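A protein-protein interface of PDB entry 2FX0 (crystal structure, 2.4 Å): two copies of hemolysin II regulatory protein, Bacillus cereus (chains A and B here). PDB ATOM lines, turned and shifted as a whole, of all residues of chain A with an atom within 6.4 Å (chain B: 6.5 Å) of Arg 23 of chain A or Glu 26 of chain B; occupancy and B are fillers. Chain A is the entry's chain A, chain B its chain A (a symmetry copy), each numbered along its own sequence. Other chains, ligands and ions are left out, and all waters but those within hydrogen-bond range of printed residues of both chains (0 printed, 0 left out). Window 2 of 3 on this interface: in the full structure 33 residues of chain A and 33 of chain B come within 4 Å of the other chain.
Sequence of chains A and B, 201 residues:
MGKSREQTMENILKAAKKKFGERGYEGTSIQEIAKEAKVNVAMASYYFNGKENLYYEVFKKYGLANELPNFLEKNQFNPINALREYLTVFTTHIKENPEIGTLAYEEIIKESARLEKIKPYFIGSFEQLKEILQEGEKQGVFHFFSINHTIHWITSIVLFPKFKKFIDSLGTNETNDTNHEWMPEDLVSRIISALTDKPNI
NZ of Lys 18 of chain A lies within salt-bridge range of OE2 of Glu 22 of chain A (3.3 Å). The side-chain amino group (NZ) of Lys 19 of chain A is in salt-bridge range of the side-chain carboxylate (OE1) of Glu 22 of chain A, at 3.4 Å. The side-chain carboxylate (OE1) of Glu 22 of chain A lies within salt-bridge range of the guanidinium group (NH1) of Arg 23 of chain A, at 3.7 Å. NH2 of Arg 114 of chain B lies within salt-bridge range of OE2 of Glu 26 of chain B, at 3.2 Å.
Of the 14 printed residues of chain A, 4 touch a printed residue of chain B. Printed residues of chain A that touch a printed residue of chain B: Glu 22, Arg 23, Glu 26 and Gly 27. Among the printed residues, no Asp or Glu carboxylate lies within 4 Å of a Lys or Arg side-chain nitrogen of the other chain.
The guanidinium group of Arg 23 of chain A lies within hydrogen-bond range of the backbone carbonyl oxygen of Glu 26 of chain B. The backbone carbonyl oxygen (O) of Glu 26 of chain A is in hydrogen-bond range of the guanidinium group (NE) of Arg 23 of chain B (3.4 Å).
Among the printed residues, merely in contact across the chains: Glu 22 of chain A with Glu 26 of chain B (3.4 Å), Gly 27 of chain A with Gly 27 of chain B (3.6 Å) and Arg 23 of chain A with Arg 23 of chain B (3.8 Å).
Arg 23 of chain B touches its own counterpart, Arg 23 of chain A. Arg 23 of chain A touches Glu 26 of chain B, and with the chains exchanged Glu 26 of chain A touches Arg 23 of chain B. Gly 27 of chain A touches its own counterpart, Gly 27 of chain B. Positions printed for both chains: 20, 23, 24, 25, 26, 27, 28 and 29. Of the 5 pairs that touch across the chains among the printed residues, 4 have their exchanged pair printed and touching as well.
Of chain B, only Arg 23 (3.8 Å) and Glu 26 (3.4 Å) come within 4 Å of Arg 23 of chain A. Glu 26 of chain B touches just these residues of chain A: Glu 22 (3.4 Å) and Arg 23 (3.4 Å). Of the printed residues of chain B, Gly 27 of chain A touches Gly 27 (3.6 Å). Printed residues of chain B within 4 Å of Glu 22 of chain A: Glu 26 (3.4 Å). Arg 114 of chain B touches none of the printed residues of chain A. The nearest residue of chain B that does not touch Arg 23 of chain A is Gly 27 of chain B (4.3 Å).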
ATOM      1  N   LYS A  18     -31.215   8.894   3.914  1.00  0.00           N
ATOM      2  CA  LYS A  18     -29.833   9.112   3.492  1.00  0.00           C
ATOM      3  C   LYS A  18     -29.509   8.389   2.185  1.00  0.00           C
ATOM      4  O   LYS A  18     -29.016   9.004   1.241  1.00  0.00           O
ATOM      5  CB  LYS A  18     -28.875   8.669   4.602  1.00  0.00           C
ATOM      6  CG  LYS A  18     -27.401   8.855   4.289  1.00  0.00           C
ATOM      7  CD  LYS A  18     -26.530   8.377   5.447  1.00  0.00           C
ATOM      8  CE  LYS A  18     -25.087   8.868   5.324  1.00  0.00           C
ATOM      9  NZ  LYS A  18     -24.244   7.965   4.480  1.00  0.00           N
ATOM     10  N   LYS A  19     -29.786   7.089   2.129  1.00  0.00           N
ATOM     11  CA  LYS A  19     -29.413   6.277   0.979  1.00  0.00           C
ATOM     12  C   LYS A  19     -30.260   6.586  -0.255  1.00  0.00           C
ATOM     13  O   LYS A  19     -29.737   6.605  -1.380  1.00  0.00           O
ATOM     14  CB  LYS A  19     -29.466   4.790   1.329  1.00  0.00           C
ATOM     15  CG  LYS A  19     -28.462   4.361   2.422  1.00  0.00           C
ATOM     16  CD  LYS A  19     -27.082   4.143   1.827  1.00  0.00           C
ATOM     17  CE  LYS A  19     -25.971   4.338   2.846  1.00  0.00           C
ATOM     18  NZ  LYS A  19     -24.646   4.548   2.175  1.00  0.00           N
ATOM     19  N   PHE A  20     -31.554   6.837  -0.035  1.00  0.00           N
ATOM     20  CA  PHE A  20     -32.481   7.179  -1.104  1.00  0.00           C
ATOM     21  C   PHE A  20     -32.124   8.536  -1.649  1.00  0.00           C
ATOM     22  O   PHE A  20     -32.162   8.748  -2.857  1.00  0.00           O
ATOM     23  CB  PHE A  20     -33.937   7.188  -0.621  1.00  0.00           C
ATOM     24  CG  PHE A  20     -34.594   5.827  -0.601  1.00  0.00           C
ATOM     25  CD1 PHE A  20     -34.583   5.009  -1.732  1.00  0.00           C
ATOM     26  CD2 PHE A  20     -35.252   5.374   0.541  1.00  0.00           C
ATOM     27  CE1 PHE A  20     -35.212   3.765  -1.718  1.00  0.00           C
ATOM     28  CE2 PHE A  20     -35.890   4.128   0.562  1.00  0.00           C
ATOM     29  CZ  PHE A  20     -35.871   3.327  -0.564  1.00  0.00           C
ATOM     30  N   GLY A  21     -31.776   9.451  -0.747  1.00  0.00           N
ATOM     31  CA  GLY A  21     -31.284  10.763  -1.121  1.00  0.00           C
ATOM     32  C   GLY A  21     -30.019  10.664  -1.955  1.00  0.00           C
ATOM     33  O   GLY A  21     -29.828  11.448  -2.873  1.00  0.00           O
ATOM     34  N   GLU A  22     -29.160   9.698  -1.645  1.00  0.00           N
ATOM     35  CA  GLU A  22     -27.918   9.507  -2.401  1.00  0.00           C
ATOM     36  C   GLU A  22     -28.139   8.895  -3.787  1.00  0.00           C
ATOM     37  O   GLU A  22     -27.661   9.430  -4.779  1.00  0.00           O
ATOM     38  CB  GLU A  22     -26.914   8.647  -1.602  1.00  0.00           C
ATOM     39  CG  GLU A  22     -26.226   9.381  -0.448  1.00  0.00           C
ATOM     40  CD  GLU A  22     -25.428   8.468   0.485  1.00  0.00           C
ATOM     41  OE1 GLU A  22     -25.426   7.223   0.315  1.00  0.00           O
ATOM     42  OE2 GLU A  22     -24.794   9.017   1.408  1.00  0.00           O
ATOM     43  N   ARG A  23     -28.866   7.781  -3.844  1.00  0.00           N
ATOM     44  CA  ARG A  23     -28.908   6.928  -5.037  1.00  0.00           C
ATOM     45  C   ARG A  23     -30.241   6.894  -5.790  1.00  0.00           C
ATOM     46  O   ARG A  23     -30.331   6.295  -6.862  1.00  0.00           O
ATOM     47  CB  ARG A  23     -28.523   5.492  -4.661  1.00  0.00           C
ATOM     48  CG  ARG A  23     -27.035   5.214  -4.624  1.00  0.00           C
ATOM     49  CD  ARG A  23     -26.771   3.777  -4.158  1.00  0.00           C
ATOM     50  NE  ARG A  23     -25.347   3.442  -4.158  1.00  0.00           N
ATOM     51  CZ  ARG A  23     -24.477   3.887  -3.255  1.00  0.00           C
ATOM     52  NH1 ARG A  23     -24.881   4.687  -2.273  1.00  0.00           N
ATOM     53  NH2 ARG A  23     -23.201   3.538  -3.334  1.00  0.00           N
ATOM     54  N   GLY A  24     -31.276   7.512  -5.229  1.00  0.00           N
ATOM     55  CA  GLY A  24     -32.619   7.423  -5.799  1.00  0.00           C
ATOM     56  C   GLY A  24     -33.274   6.089  -5.500  1.00  0.00           C
ATOM     57  O   GLY A  24     -32.608   5.152  -5.053  1.00  0.00           O
ATOM     58  N   TYR A  25     -34.577   6.000  -5.753  1.00  0.00           N
ATOM     59  CA  TYR A  25     -35.351   4.810  -5.440  1.00  0.00           C
ATOM     60  C   TYR A  25     -34.771   3.537  -6.061  1.00  0.00           C
ATOM     61  O   TYR A  25     -34.410   2.580  -5.350  1.00  0.00           O
ATOM     62  CB  TYR A  25     -36.822   4.981  -5.852  1.00  0.00           C
ATOM     63  CG  TYR A  25     -37.651   3.750  -5.570  1.00  0.00           C
ATOM     64  CD1 TYR A  25     -38.099   3.465  -4.278  1.00  0.00           C
ATOM     65  CD2 TYR A  25     -37.952   2.846  -6.588  1.00  0.00           C
ATOM     66  CE1 TYR A  25     -38.845   2.329  -4.018  1.00  0.00           C
ATOM     67  CE2 TYR A  25     -38.692   1.700  -6.330  1.00  0.00           C
ATOM     68  CZ  TYR A  25     -39.133   1.451  -5.051  1.00  0.00           C
ATOM     69  OH  TYR A  25     -39.868   0.316  -4.819  1.00  0.00           O
ATOM     70  N   GLU A  26     -34.683   3.539  -7.384  1.00  0.00           N
ATOM     71  CA  GLU A  26     -34.248   2.368  -8.138  1.00  0.00           C
ATOM     72  C   GLU A  26     -32.755   2.084  -7.952  1.00  0.00           C
ATOM     73  O   GLU A  26     -32.308   0.953  -8.168  1.00  0.00           O
ATOM     74  CB  GLU A  26     -34.626   2.495  -9.625  1.00  0.00           C
ATOM     75  CG  GLU A  26     -34.283   3.844 -10.250  1.00  0.00           C
ATOM     76  CD  GLU A  26     -35.197   4.978  -9.795  1.00  0.00           C
ATOM     77  OE1 GLU A  26     -34.682   6.082  -9.492  1.00  0.00           O
ATOM     78  OE2 GLU A  26     -36.429   4.766  -9.740  1.00  0.00           O
ATOM     79  N   GLY A  27     -32.006   3.099  -7.515  1.00  0.00           N
ATOM     80  CA  GLY A  27     -30.576   2.954  -7.224  1.00  0.00           C
ATOM     81  C   GLY A  27     -30.194   2.371  -5.866  1.00  0.00           C
ATOM     82  O   GLY A  27     -29.058   1.916  -5.683  1.00  0.00           O
ATOM     83  N   THR A  28     -31.139   2.382  -4.923  1.00  0.00           N
ATOM     84  CA  THR A  28     -30.910   1.918  -3.544  1.00  0.00           C
ATOM     85  C   THR A  28     -31.546   0.550  -3.287  1.00  0.00           C
ATOM     86  O   THR A  28     -32.677   0.292  -3.687  1.00  0.00           O
ATOM     87  CB  THR A  28     -31.497   2.912  -2.504  1.00  0.00           C
ATOM     88  OG1 THR A  28     -31.099   4.249  -2.827  1.00  0.00           O
ATOM     89  CG2 THR A  28     -31.017   2.589  -1.112  1.00  0.00           C
ATOM     90  N   SER A  29     -30.820  -0.323  -2.607  1.00  0.00           N
ATOM     91  CA  SER A  29     -31.370  -1.602  -2.189  1.00  0.00           C
ATOM     92  C   SER A  29     -31.752  -1.533  -0.716  1.00  0.00           C
ATOM     93  O   SER A  29     -31.201  -0.728   0.048  1.00  0.00           O
ATOM     94  CB  SER A  29     -30.348  -2.715  -2.406  1.00  0.00           C
ATOM     95  OG  SER A  29     -29.218  -2.527  -1.570  1.00  0.00           O
ATOM     96  N   GLU A  32     -28.573  -2.111   1.431  1.00  0.00           N
ATOM     97  CA  GLU A  32     -27.730  -0.942   1.719  1.00  0.00           C
ATOM     98  C   GLU A  32     -28.296  -0.157   2.900  1.00  0.00           C
ATOM     99  O   GLU A  32     -27.550   0.309   3.763  1.00  0.00           O
ATOM    100  CB  GLU A  32     -27.647  -0.010   0.511  1.00  0.00           C
ATOM    101  CG  GLU A  32     -26.908  -0.566  -0.682  1.00  0.00           C
ATOM    102  CD  GLU A  32     -27.162   0.222  -1.973  1.00  0.00           C
ATOM    103  OE1 GLU A  32     -26.642  -0.206  -3.027  1.00  0.00           O
ATOM    104  OE2 GLU A  32     -27.881   1.257  -1.941  1.00  0.00           O
ATOM    105  N   THR A 102     -32.777  15.612  -4.500  1.00  0.00           N
ATOM    106  CA  THR A 102     -32.760  14.405  -5.337  1.00  0.00           C
ATOM    107  C   THR A 102     -34.141  13.763  -5.484  1.00  0.00           C
ATOM    108  O   THR A 102     -34.534  13.392  -6.590  1.00  0.00           O
ATOM    109  CB  THR A 102     -31.724  13.388  -4.802  1.00  0.00           C
ATOM    110  OG1 THR A 102     -30.426  13.997  -4.821  1.00  0.00           O
ATOM    111  CG2 THR A 102     -31.691  12.095  -5.638  1.00  0.00           C
ATOM    112  N   PHE B  20     -28.078   3.897 -17.096  1.00  0.00           N
ATOM    113  CA  PHE B  20     -27.775   5.155 -16.430  1.00  0.00           C
ATOM    114  C   PHE B  20     -29.001   6.028 -16.445  1.00  0.00           C
ATOM    115  O   PHE B  20     -29.304   6.690 -15.458  1.00  0.00           O
ATOM    116  CB  PHE B  20     -26.611   5.896 -17.101  1.00  0.00           C
ATOM    117  CG  PHE B  20     -25.242   5.430 -16.661  1.00  0.00           C
ATOM    118  CD1 PHE B  20     -24.908   5.364 -15.308  1.00  0.00           C
ATOM    119  CD2 PHE B  20     -24.273   5.086 -17.603  1.00  0.00           C
ATOM    120  CE1 PHE B  20     -23.636   4.958 -14.906  1.00  0.00           C
ATOM    121  CE2 PHE B  20     -22.992   4.683 -17.209  1.00  0.00           C
ATOM    122  CZ  PHE B  20     -22.674   4.621 -15.865  1.00  0.00           C
ATOM    123  N   ARG B  23     -31.314   4.360 -13.640  1.00  0.00           N
ATOM    124  CA  ARG B  23     -30.928   4.330 -12.225  1.00  0.00           C
ATOM    125  C   ARG B  23     -30.028   5.475 -11.752  1.00  0.00           C
ATOM    126  O   ARG B  23     -29.750   5.590 -10.558  1.00  0.00           O
ATOM    127  CB  ARG B  23     -30.235   3.000 -11.905  1.00  0.00           C
ATOM    128  CG  ARG B  23     -31.167   1.851 -11.583  1.00  0.00           C
ATOM    129  CD  ARG B  23     -30.367   0.561 -11.362  1.00  0.00           C
ATOM    130  NE  ARG B  23     -31.220  -0.569 -10.994  1.00  0.00           N
ATOM    131  CZ  ARG B  23     -32.012  -1.213 -11.846  1.00  0.00           C
ATOM    132  NH1 ARG B  23     -32.064  -0.845 -13.122  1.00  0.00           N
ATOM    133  NH2 ARG B  23     -32.757  -2.225 -11.425  1.00  0.00           N
ATOM    134  N   GLY B  24     -29.559   6.306 -12.678  1.00  0.00           N
ATOM    135  CA  GLY B  24     -28.587   7.347 -12.348  1.00  0.00           C
ATOM    136  C   GLY B  24     -27.191   6.782 -12.168  1.00  0.00           C
ATOM    137  O   GLY B  24     -27.017   5.565 -12.073  1.00  0.00           O
ATOM    138  N   TYR B  25     -26.198   7.666 -12.116  1.00  0.00           N
ATOM    139  CA  TYR B  25     -24.803   7.263 -12.028  1.00  0.00           C
ATOM    140  C   TYR B  25     -24.522   6.327 -10.851  1.00  0.00           C
ATOM    141  O   TYR B  25     -24.063   5.184 -11.032  1.00  0.00           O
ATOM    142  CB  TYR B  25     -23.877   8.489 -11.967  1.00  0.00           C
ATOM    143  CG  TYR B  25     -22.420   8.110 -11.844  1.00  0.00           C
ATOM    144  CD1 TYR B  25     -21.692   7.677 -12.956  1.00  0.00           C
ATOM    145  CD2 TYR B  25     -21.778   8.141 -10.607  1.00  0.00           C
ATOM    146  CE1 TYR B  25     -20.362   7.315 -12.838  1.00  0.00           C
ATOM    147  CE2 TYR B  25     -20.446   7.769 -10.482  1.00  0.00           C
ATOM    148  CZ  TYR B  25     -19.750   7.360 -11.596  1.00  0.00           C
ATOM    149  OH  TYR B  25     -18.433   7.004 -11.452  1.00  0.00           O
ATOM    150  N   GLU B  26     -24.802   6.820  -9.652  1.00  0.00           N
ATOM    151  CA  GLU B  26     -24.500   6.097  -8.422  1.00  0.00           C
ATOM    152  C   GLU B  26     -25.407   4.879  -8.229  1.00  0.00           C
ATOM    153  O   GLU B  26     -25.051   3.952  -7.495  1.00  0.00           O
ATOM    154  CB  GLU B  26     -24.537   7.038  -7.204  1.00  0.00           C
ATOM    155  CG  GLU B  26     -25.761   7.948  -7.147  1.00  0.00           C
ATOM    156  CD  GLU B  26     -25.731   9.078  -8.172  1.00  0.00           C
ATOM    157  OE1 GLU B  26     -26.776   9.335  -8.818  1.00  0.00           O
ATOM    158  OE2 GLU B  26     -24.661   9.709  -8.332  1.00  0.00           O
ATOM    159  N   GLY B  27     -26.549   4.872  -8.920  1.00  0.00           N
ATOM    160  CA  GLY B  27     -27.481   3.742  -8.890  1.00  0.00           C
ATOM    161  C   GLY B  27     -27.174   2.557  -9.803  1.00  0.00           C
ATOM    162  O   GLY B  27     -27.704   1.459  -9.595  1.00  0.00           O
ATOM    163  N   THR B  28     -26.320   2.779 -10.805  1.00  0.00           N
ATOM    164  CA  THR B  28     -25.971   1.761 -11.810  1.00  0.00           C
ATOM    165  C   THR B  28     -24.575   1.181 -11.577  1.00  0.00           C
ATOM    166  O   THR B  28     -23.627   1.906 -11.293  1.00  0.00           O
ATOM    167  CB  THR B  28     -26.001   2.349 -13.249  1.00  0.00           C
ATOM    168  OG1 THR B  28     -27.210   3.091 -13.450  1.00  0.00           O
ATOM    169  CG2 THR B  28     -25.929   1.256 -14.284  1.00  0.00           C
ATOM    170  N   SER B  29     -24.450  -0.130 -11.707  1.00  0.00           N
ATOM    171  CA  SER B  29     -23.150  -0.777 -11.640  1.00  0.00           C
ATOM    172  C   SER B  29     -22.669  -1.097 -13.050  1.00  0.00           C
ATOM    173  O   SER B  29     -23.476  -1.248 -13.979  1.00  0.00           O
ATOM    174  CB  SER B  29     -23.237  -2.060 -10.820  1.00  0.00           C
ATOM    175  OG  SER B  29     -24.069  -3.010 -11.464  1.00  0.00           O
ATOM    176  N   LYS B  51     -16.072   2.688 -14.794  1.00  0.00           N
ATOM    177  CA  LYS B  51     -17.443   3.197 -14.798  1.00  0.00           C
ATOM    178  C   LYS B  51     -17.572   4.706 -15.029  1.00  0.00           C
ATOM    179  O   LYS B  51     -18.474   5.142 -15.755  1.00  0.00           O
ATOM    180  CB  LYS B  51     -18.129   2.830 -13.488  1.00  0.00           C
ATOM    181  CG  LYS B  51     -19.565   3.299 -13.378  1.00  0.00           C
ATOM    182  CD  LYS B  51     -19.979   3.248 -11.917  1.00  0.00           C
ATOM    183  CE  LYS B  51     -21.393   3.684 -11.728  1.00  0.00           C
ATOM    184  NZ  LYS B  51     -21.692   3.849 -10.282  1.00  0.00           N
ATOM    185  N   GLU B 106     -29.939  14.918 -12.947  1.00  0.00           N
ATOM    186  CA  GLU B 106     -28.945  14.557 -11.967  1.00  0.00           C
ATOM    187  C   GLU B 106     -27.768  15.552 -12.017  1.00  0.00           C
ATOM    188  O   GLU B 106     -27.369  16.066 -10.978  1.00  0.00           O
ATOM    189  CB  GLU B 106     -28.503  13.104 -12.136  1.00  0.00           C
ATOM    190  CG  GLU B 106     -29.554  12.072 -11.716  1.00  0.00           C
ATOM    191  CD  GLU B 106     -29.814  12.073 -10.206  1.00  0.00           C
ATOM    192  OE1 GLU B 106     -28.836  12.097  -9.419  1.00  0.00           O
ATOM    193  OE2 GLU B 106     -30.994  12.046  -9.796  1.00  0.00           O
ATOM    194  N   GLU B 107     -27.281  15.886 -13.216  1.00  0.00           N
ATOM    195  CA  GLU B 107     -25.933  16.458 -13.331  1.00  0.00           C
ATOM    196  C   GLU B 107     -25.921  17.958 -13.449  1.00  0.00           C
ATOM    197  O   GLU B 107     -25.059  18.627 -12.894  1.00  0.00           O
ATOM    198  CB  GLU B 107     -25.114  15.803 -14.460  1.00  0.00           C
ATOM    199  CG  GLU B 107     -24.897  14.270 -14.292  1.00  0.00           C
ATOM    200  CD  GLU B 107     -24.046  13.875 -13.078  1.00  0.00           C
ATOM    201  OE1 GLU B 107     -23.387  14.745 -12.469  1.00  0.00           O
ATOM    202  OE2 GLU B 107     -24.025  12.679 -12.730  1.00  0.00           O
ATOM    203  N   GLU B 111     -26.963  18.351  -9.164  1.00  0.00           N
ATOM    204  CA  GLU B 111     -25.656  18.082  -8.547  1.00  0.00           C
ATOM    205  C   GLU B 111     -24.413  18.831  -9.006  1.00  0.00           C
ATOM    206  O   GLU B 111     -24.501  19.930  -9.571  1.00  0.00           O
ATOM    207  CB  GLU B 111     -25.387  16.582  -8.495  1.00  0.00           C
ATOM    208  CG  GLU B 111     -26.014  15.926  -7.284  1.00  0.00           C
ATOM    209  CD  GLU B 111     -26.175  14.424  -7.435  1.00  0.00           C
ATOM    210  OE1 GLU B 111     -26.749  13.985  -8.462  1.00  0.00           O
ATOM    211  OE2 GLU B 111     -25.736  13.692  -6.517  1.00  0.00           O
ATOM    212  N   ARG B 114     -19.270  15.275 -10.703  1.00  0.00           N
ATOM    213  CA  ARG B 114     -18.710  15.084 -12.052  1.00  0.00           C
ATOM    214  C   ARG B 114     -19.033  16.233 -13.024  1.00  0.00           C
ATOM    215  O   ARG B 114     -18.769  16.123 -14.226  1.00  0.00           O
ATOM    216  CB  ARG B 114     -19.284  13.787 -12.635  1.00  0.00           C
ATOM    217  CG  ARG B 114     -19.155  12.584 -11.702  1.00  0.00           C
ATOM    218  CD  ARG B 114     -20.083  11.434 -12.081  1.00  0.00           C
ATOM    219  NE  ARG B 114     -21.474  11.705 -11.717  1.00  0.00           N
ATOM    220  CZ  ARG B 114     -21.973  11.585 -10.488  1.00  0.00           C
ATOM    221  NH1 ARG B 114     -21.204  11.200  -9.476  1.00  0.00           N
ATOM    222  NH2 ARG B 114     -23.254  11.839 -10.272  1.00  0.00           N
